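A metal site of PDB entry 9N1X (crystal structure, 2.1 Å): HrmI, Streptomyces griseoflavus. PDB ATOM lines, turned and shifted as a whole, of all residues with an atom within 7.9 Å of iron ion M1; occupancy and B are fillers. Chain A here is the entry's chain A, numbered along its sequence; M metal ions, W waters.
Iron ion M1 is bound by water W2 (2.1 Å), the side-chain carboxylate of Asp 292 (2.1 Å), water W3 (2.1 Å), water W1 (2.2 Å), the side-chain carboxylate of Glu 258 (2.2 Å) and a ring nitrogen (ND1) of His 295 (2.2 Å).
Iron ion M1 has six donor atoms within binding distance.
Water W2 bridges OE1 of Glu 258 and OD2 of Asp 292.
The side-chain carboxylate (OE2) of Glu 258 lies close to the side-chain amide nitrogen (ND2) of Asn 190 (3.1 Å).
ND1 of His 295 sits close to ND2 of Asn 190, at 3.4 Å.
The side-chain carboxylate of Asp 193 sits at hydrogen-bond distance from a ring nitrogen (NE2) of His 295 (2.7 Å).
Residues that only touch iron ion M1: Asn 190 (3.8 Å) and Glu 194 (3.8 Å).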
ATOM      1  N   PHE A 168      24.402  24.517  35.219  1.00  0.00           N
ATOM      2  CA  PHE A 168      23.673  23.551  34.406  1.00  0.00           C
ATOM      3  C   PHE A 168      24.618  22.676  33.584  1.00  0.00           C
ATOM      4  O   PHE A 168      24.401  21.472  33.428  1.00  0.00           O
ATOM      5  CB  PHE A 168      22.710  24.293  33.482  1.00  0.00           C
ATOM      6  CG  PHE A 168      21.355  23.688  33.393  1.00  0.00           C
ATOM      7  CD1 PHE A 168      20.400  23.939  34.370  1.00  0.00           C
ATOM      8  CD2 PHE A 168      21.016  22.874  32.325  1.00  0.00           C
ATOM      9  CE1 PHE A 168      19.142  23.381  34.278  1.00  0.00           C
ATOM     10  CE2 PHE A 168      19.766  22.320  32.228  1.00  0.00           C
ATOM     11  CZ  PHE A 168      18.818  22.560  33.210  1.00  0.00           C
ATOM     12  N   LEU A 172      24.918  18.516  33.893  1.00  0.00           N
ATOM     13  CA  LEU A 172      24.757  17.572  32.787  1.00  0.00           C
ATOM     14  C   LEU A 172      25.994  16.695  32.639  1.00  0.00           C
ATOM     15  O   LEU A 172      25.890  15.497  32.355  1.00  0.00           O
ATOM     16  CB  LEU A 172      24.466  18.305  31.483  1.00  0.00           C
ATOM     17  CG  LEU A 172      23.162  19.100  31.423  1.00  0.00           C
ATOM     18  CD1 LEU A 172      23.187  20.054  30.247  1.00  0.00           C
ATOM     19  CD2 LEU A 172      21.991  18.162  31.303  1.00  0.00           C
ATOM     20  N   ASN A 190      22.843  18.061  24.774  1.00  0.00           N
ATOM     21  CA  ASN A 190      22.332  19.118  25.634  1.00  0.00           C
ATOM     22  C   ASN A 190      23.485  19.917  26.246  1.00  0.00           C
ATOM     23  O   ASN A 190      23.511  21.154  26.173  1.00  0.00           O
ATOM     24  CB  ASN A 190      21.432  18.498  26.706  1.00  0.00           C
ATOM     25  CG  ASN A 190      20.565  19.522  27.431  1.00  0.00           C
ATOM     26  OD1 ASN A 190      21.055  20.574  27.831  1.00  0.00           O
ATOM     27  ND2 ASN A 190      19.289  19.201  27.620  1.00  0.00           N
ATOM     28  N   TYR A 191      24.468  19.215  26.825  1.00  0.00           N
ATOM     29  CA  TYR A 191      25.680  19.888  27.326  1.00  0.00           C
ATOM     30  C   TYR A 191      26.360  20.713  26.237  1.00  0.00           C
ATOM     31  O   TYR A 191      26.744  21.870  26.457  1.00  0.00           O
ATOM     32  CB  TYR A 191      26.621  18.828  27.906  1.00  0.00           C
ATOM     33  CG  TYR A 191      28.048  19.281  28.141  1.00  0.00           C
ATOM     34  CD1 TYR A 191      28.403  19.873  29.346  1.00  0.00           C
ATOM     35  CD2 TYR A 191      29.039  19.086  27.172  1.00  0.00           C
ATOM     36  CE1 TYR A 191      29.704  20.294  29.584  1.00  0.00           C
ATOM     37  CE2 TYR A 191      30.361  19.512  27.407  1.00  0.00           C
ATOM     38  CZ  TYR A 191      30.679  20.108  28.616  1.00  0.00           C
ATOM     39  OH  TYR A 191      31.953  20.525  28.887  1.00  0.00           O
ATOM     40  N   ASP A 193      25.031  22.130  23.695  1.00  0.00           N
ATOM     41  CA  ASP A 193      24.233  23.346  23.523  1.00  0.00           C
ATOM     42  C   ASP A 193      24.529  24.347  24.649  1.00  0.00           C
ATOM     43  O   ASP A 193      24.689  25.535  24.395  1.00  0.00           O
ATOM     44  CB  ASP A 193      22.733  23.020  23.488  1.00  0.00           C
ATOM     45  CG  ASP A 193      22.278  22.332  22.201  1.00  0.00           C
ATOM     46  OD1 ASP A 193      22.940  22.405  21.133  1.00  0.00           O
ATOM     47  OD2 ASP A 193      21.199  21.691  22.260  1.00  0.00           O
ATOM     48  N   GLU A 194      24.579  23.869  25.898  1.00  0.00           N
ATOM     49  CA  GLU A 194      24.932  24.729  27.029  1.00  0.00           C
ATOM     50  C   GLU A 194      26.291  25.399  26.817  1.00  0.00           C
ATOM     51  O   GLU A 194      26.527  26.519  27.278  1.00  0.00           O
ATOM     52  CB  GLU A 194      24.942  23.929  28.337  1.00  0.00           C
ATOM     53  CG  GLU A 194      23.561  23.474  28.828  1.00  0.00           C
ATOM     54  CD  GLU A 194      22.665  24.640  29.229  1.00  0.00           C
ATOM     55  OE1 GLU A 194      23.120  25.494  30.031  1.00  0.00           O
ATOM     56  OE2 GLU A 194      21.515  24.722  28.751  1.00  0.00           O
ATOM     57  N   HIS A 204      25.898  29.308  27.877  1.00  0.00           N
ATOM     58  CA  HIS A 204      24.721  29.718  28.649  1.00  0.00           C
ATOM     59  C   HIS A 204      25.086  30.392  29.966  1.00  0.00           C
ATOM     60  O   HIS A 204      24.435  31.353  30.363  1.00  0.00           O
ATOM     61  CB  HIS A 204      23.810  28.527  28.880  1.00  0.00           C
ATOM     62  CG  HIS A 204      23.055  28.120  27.667  1.00  0.00           C
ATOM     63  ND1 HIS A 204      22.150  27.079  27.664  1.00  0.00           N
ATOM     64  CD2 HIS A 204      23.087  28.593  26.403  1.00  0.00           C
ATOM     65  CE1 HIS A 204      21.655  26.935  26.451  1.00  0.00           C
ATOM     66  NE2 HIS A 204      22.199  27.852  25.670  1.00  0.00           N
ATOM     67  N   PHE A 254      15.729  16.947  36.355  1.00  0.00           N
ATOM     68  CA  PHE A 254      16.074  17.887  35.310  1.00  0.00           C
ATOM     69  C   PHE A 254      15.213  17.705  34.071  1.00  0.00           C
ATOM     70  O   PHE A 254      15.095  18.642  33.277  1.00  0.00           O
ATOM     71  CB  PHE A 254      17.564  17.792  34.998  1.00  0.00           C
ATOM     72  CG  PHE A 254      18.430  18.059  36.237  1.00  0.00           C
ATOM     73  CD1 PHE A 254      18.570  19.356  36.730  1.00  0.00           C
ATOM     74  CD2 PHE A 254      19.057  17.021  36.929  1.00  0.00           C
ATOM     75  CE1 PHE A 254      19.310  19.603  37.872  1.00  0.00           C
ATOM     76  CE2 PHE A 254      19.815  17.278  38.084  1.00  0.00           C
ATOM     77  CZ  PHE A 254      19.938  18.569  38.551  1.00  0.00           C
ATOM     78  N   THR A 257      12.678  20.145  34.811  1.00  0.00           N
ATOM     79  CA  THR A 257      13.258  21.451  34.557  1.00  0.00           C
ATOM     80  C   THR A 257      13.156  21.853  33.088  1.00  0.00           C
ATOM     81  O   THR A 257      12.627  22.926  32.764  1.00  0.00           O
ATOM     82  CB  THR A 257      14.710  21.463  35.020  1.00  0.00           C
ATOM     83  OG1 THR A 257      14.744  21.237  36.436  1.00  0.00           O
ATOM     84  CG2 THR A 257      15.374  22.780  34.675  1.00  0.00           C
ATOM     85  N   GLU A 258      13.631  20.997  32.179  1.00  0.00           N
ATOM     86  CA  GLU A 258      13.560  21.313  30.759  1.00  0.00           C
ATOM     87  C   GLU A 258      12.131  21.484  30.300  1.00  0.00           C
ATOM     88  O   GLU A 258      11.809  22.401  29.536  1.00  0.00           O
ATOM     89  CB  GLU A 258      14.248  20.206  29.941  1.00  0.00           C
ATOM     90  CG  GLU A 258      15.711  19.947  30.329  1.00  0.00           C
ATOM     91  CD  GLU A 258      16.591  21.155  30.062  1.00  0.00           C
ATOM     92  OE1 GLU A 258      16.552  22.109  30.877  1.00  0.00           O
ATOM     93  OE2 GLU A 258      17.309  21.168  29.041  1.00  0.00           O
ATOM     94  N   TYR A 259      11.242  20.591  30.740  1.00  0.00           N
ATOM     95  CA  TYR A 259       9.838  20.650  30.344  1.00  0.00           C
ATOM     96  C   TYR A 259       9.196  21.985  30.704  1.00  0.00           C
ATOM     97  O   TYR A 259       8.441  22.550  29.903  1.00  0.00           O
ATOM     98  CB  TYR A 259       9.099  19.493  31.013  1.00  0.00           C
ATOM     99  CG  TYR A 259       7.659  19.286  30.605  1.00  0.00           C
ATOM    100  CD1 TYR A 259       7.288  19.181  29.262  1.00  0.00           C
ATOM    101  CD2 TYR A 259       6.673  19.163  31.572  1.00  0.00           C
ATOM    102  CE1 TYR A 259       5.950  18.963  28.900  1.00  0.00           C
ATOM    103  CE2 TYR A 259       5.341  18.944  31.218  1.00  0.00           C
ATOM    104  CZ  TYR A 259       4.996  18.838  29.893  1.00  0.00           C
ATOM    105  OH  TYR A 259       3.669  18.621  29.600  1.00  0.00           O
ATOM    106  N   VAL A 261      10.667  25.018  31.518  1.00  0.00           N
ATOM    107  CA  VAL A 261      11.360  26.295  31.245  1.00  0.00           C
ATOM    108  C   VAL A 261      10.645  27.127  30.193  1.00  0.00           C
ATOM    109  O   VAL A 261      10.501  28.346  30.394  1.00  0.00           O
ATOM    110  CB  VAL A 261      12.833  26.044  30.915  1.00  0.00           C
ATOM    111  CG1 VAL A 261      13.423  27.239  30.151  1.00  0.00           C
ATOM    112  CG2 VAL A 261      13.616  25.797  32.195  1.00  0.00           C
ATOM    113  N   HIS A 288      16.375  30.095  25.575  1.00  0.00           N
ATOM    114  CA  HIS A 288      15.817  28.891  26.182  1.00  0.00           C
ATOM    115  C   HIS A 288      14.373  28.638  25.780  1.00  0.00           C
ATOM    116  O   HIS A 288      13.945  27.478  25.749  1.00  0.00           O
ATOM    117  CB  HIS A 288      15.940  28.978  27.691  1.00  0.00           C
ATOM    118  CG  HIS A 288      17.339  28.786  28.169  1.00  0.00           C
ATOM    119  ND1 HIS A 288      18.292  29.769  28.046  1.00  0.00           N
ATOM    120  CD2 HIS A 288      17.972  27.705  28.668  1.00  0.00           C
ATOM    121  CE1 HIS A 288      19.446  29.319  28.513  1.00  0.00           C
ATOM    122  NE2 HIS A 288      19.282  28.060  28.885  1.00  0.00           N
ATOM    123  N   ILE A 291      14.983  26.764  22.648  1.00  0.00           N
ATOM    124  CA  ILE A 291      15.915  25.642  22.823  1.00  0.00           C
ATOM    125  C   ILE A 291      15.296  24.555  23.696  1.00  0.00           C
ATOM    126  O   ILE A 291      15.382  23.361  23.391  1.00  0.00           O
ATOM    127  CB  ILE A 291      17.245  26.159  23.406  1.00  0.00           C
ATOM    128  CG1 ILE A 291      18.013  26.973  22.361  1.00  0.00           C
ATOM    129  CG2 ILE A 291      18.094  25.016  23.902  1.00  0.00           C
ATOM    130  N   ASP A 292      14.614  24.945  24.768  1.00  0.00           N
ATOM    131  CA  ASP A 292      14.190  23.960  25.751  1.00  0.00           C
ATOM    132  C   ASP A 292      12.900  23.232  25.379  1.00  0.00           C
ATOM    133  O   ASP A 292      12.593  22.210  26.003  1.00  0.00           O
ATOM    134  CB  ASP A 292      14.088  24.618  27.126  1.00  0.00           C
ATOM    135  CG  ASP A 292      15.417  24.592  27.848  1.00  0.00           C
ATOM    136  OD1 ASP A 292      16.277  23.754  27.464  1.00  0.00           O
ATOM    137  OD2 ASP A 292      15.607  25.382  28.784  1.00  0.00           O
ATOM    138  N   ALA A 293      12.150  23.704  24.375  1.00  0.00           N
ATOM    139  CA  ALA A 293      11.133  22.838  23.772  1.00  0.00           C
ATOM    140  C   ALA A 293      11.782  21.641  23.083  1.00  0.00           C
ATOM    141  O   ALA A 293      11.251  20.526  23.130  1.00  0.00           O
ATOM    142  CB  ALA A 293      10.291  23.633  22.775  1.00  0.00           C
ATOM    143  N   VAL A 294      12.930  21.863  22.447  1.00  0.00           N
ATOM    144  CA  VAL A 294      13.658  20.761  21.830  1.00  0.00           C
ATOM    145  C   VAL A 294      14.358  19.924  22.893  1.00  0.00           C
ATOM    146  O   VAL A 294      14.338  18.688  22.832  1.00  0.00           O
ATOM    147  CB  VAL A 294      14.655  21.314  20.784  1.00  0.00           C
ATOM    148  CG1 VAL A 294      15.435  20.188  20.136  1.00  0.00           C
ATOM    149  CG2 VAL A 294      13.883  22.113  19.708  1.00  0.00           C
ATOM    150  N   HIS A 295      14.962  20.566  23.896  1.00  0.00           N
ATOM    151  CA  HIS A 295      15.619  19.797  24.955  1.00  0.00           C
ATOM    152  C   HIS A 295      14.619  18.908  25.691  1.00  0.00           C
ATOM    153  O   HIS A 295      14.929  17.752  26.005  1.00  0.00           O
ATOM    154  CB  HIS A 295      16.342  20.720  25.933  1.00  0.00           C
ATOM    155  CG  HIS A 295      17.670  21.211  25.439  1.00  0.00           C
ATOM    156  ND1 HIS A 295      18.446  22.091  26.146  1.00  0.00           N
ATOM    157  CD2 HIS A 295      18.344  20.953  24.283  1.00  0.00           C
ATOM    158  CE1 HIS A 295      19.546  22.351  25.464  1.00  0.00           C
ATOM    159  NE2 HIS A 295      19.505  21.679  24.330  1.00  0.00           N
ATOM    160  N   ALA A 296      13.422  19.442  25.999  1.00  0.00           N
ATOM    161  CA  ALA A 296      12.427  18.663  26.727  1.00  0.00           C
ATOM    162  C   ALA A 296      11.966  17.463  25.912  1.00  0.00           C
ATOM    163  O   ALA A 296      11.881  16.339  26.430  1.00  0.00           O
ATOM    164  CB  ALA A 296      11.210  19.530  27.078  1.00  0.00           C
ATOM    165  N   TRP A 299      14.715  14.990  25.809  1.00  0.00           N
ATOM    166  CA  TRP A 299      14.937  14.373  27.115  1.00  0.00           C
ATOM    167  C   TRP A 299      13.935  13.256  27.368  1.00  0.00           C
ATOM    168  O   TRP A 299      14.300  12.166  27.831  1.00  0.00           O
ATOM    169  CB  TRP A 299      14.843  15.442  28.202  1.00  0.00           C
ATOM    170  CG  TRP A 299      15.412  14.990  29.522  1.00  0.00           C
ATOM    171  CD1 TRP A 299      14.747  14.306  30.511  1.00  0.00           C
ATOM    172  CD2 TRP A 299      16.739  15.199  30.008  1.00  0.00           C
ATOM    173  NE1 TRP A 299      15.591  14.073  31.577  1.00  0.00           N
ATOM    174  CE2 TRP A 299      16.816  14.618  31.293  1.00  0.00           C
ATOM    175  CE3 TRP A 299      17.869  15.839  29.481  1.00  0.00           C
ATOM    176  CZ2 TRP A 299      17.995  14.647  32.068  1.00  0.00           C
ATOM    177  CZ3 TRP A 299      19.035  15.857  30.250  1.00  0.00           C
ATOM    178  CH2 TRP A 299      19.080  15.266  31.521  1.00  0.00           C
HETATM  179 FE    FE M   1      18.121  23.041  28.157  1.00  0.00          FE
HETATM  180 FE    FE M   2      20.745  26.489  29.325  1.00  0.00          FE
HETATM  181  O   HOH W   1      18.921  24.987  27.440  1.00  0.00           O
HETATM  182  O   HOH W   2      17.593  24.056  29.903  1.00  0.00           O
HETATM  183  O   HOH W   3      19.966  22.418  28.971  1.00  0.00           O
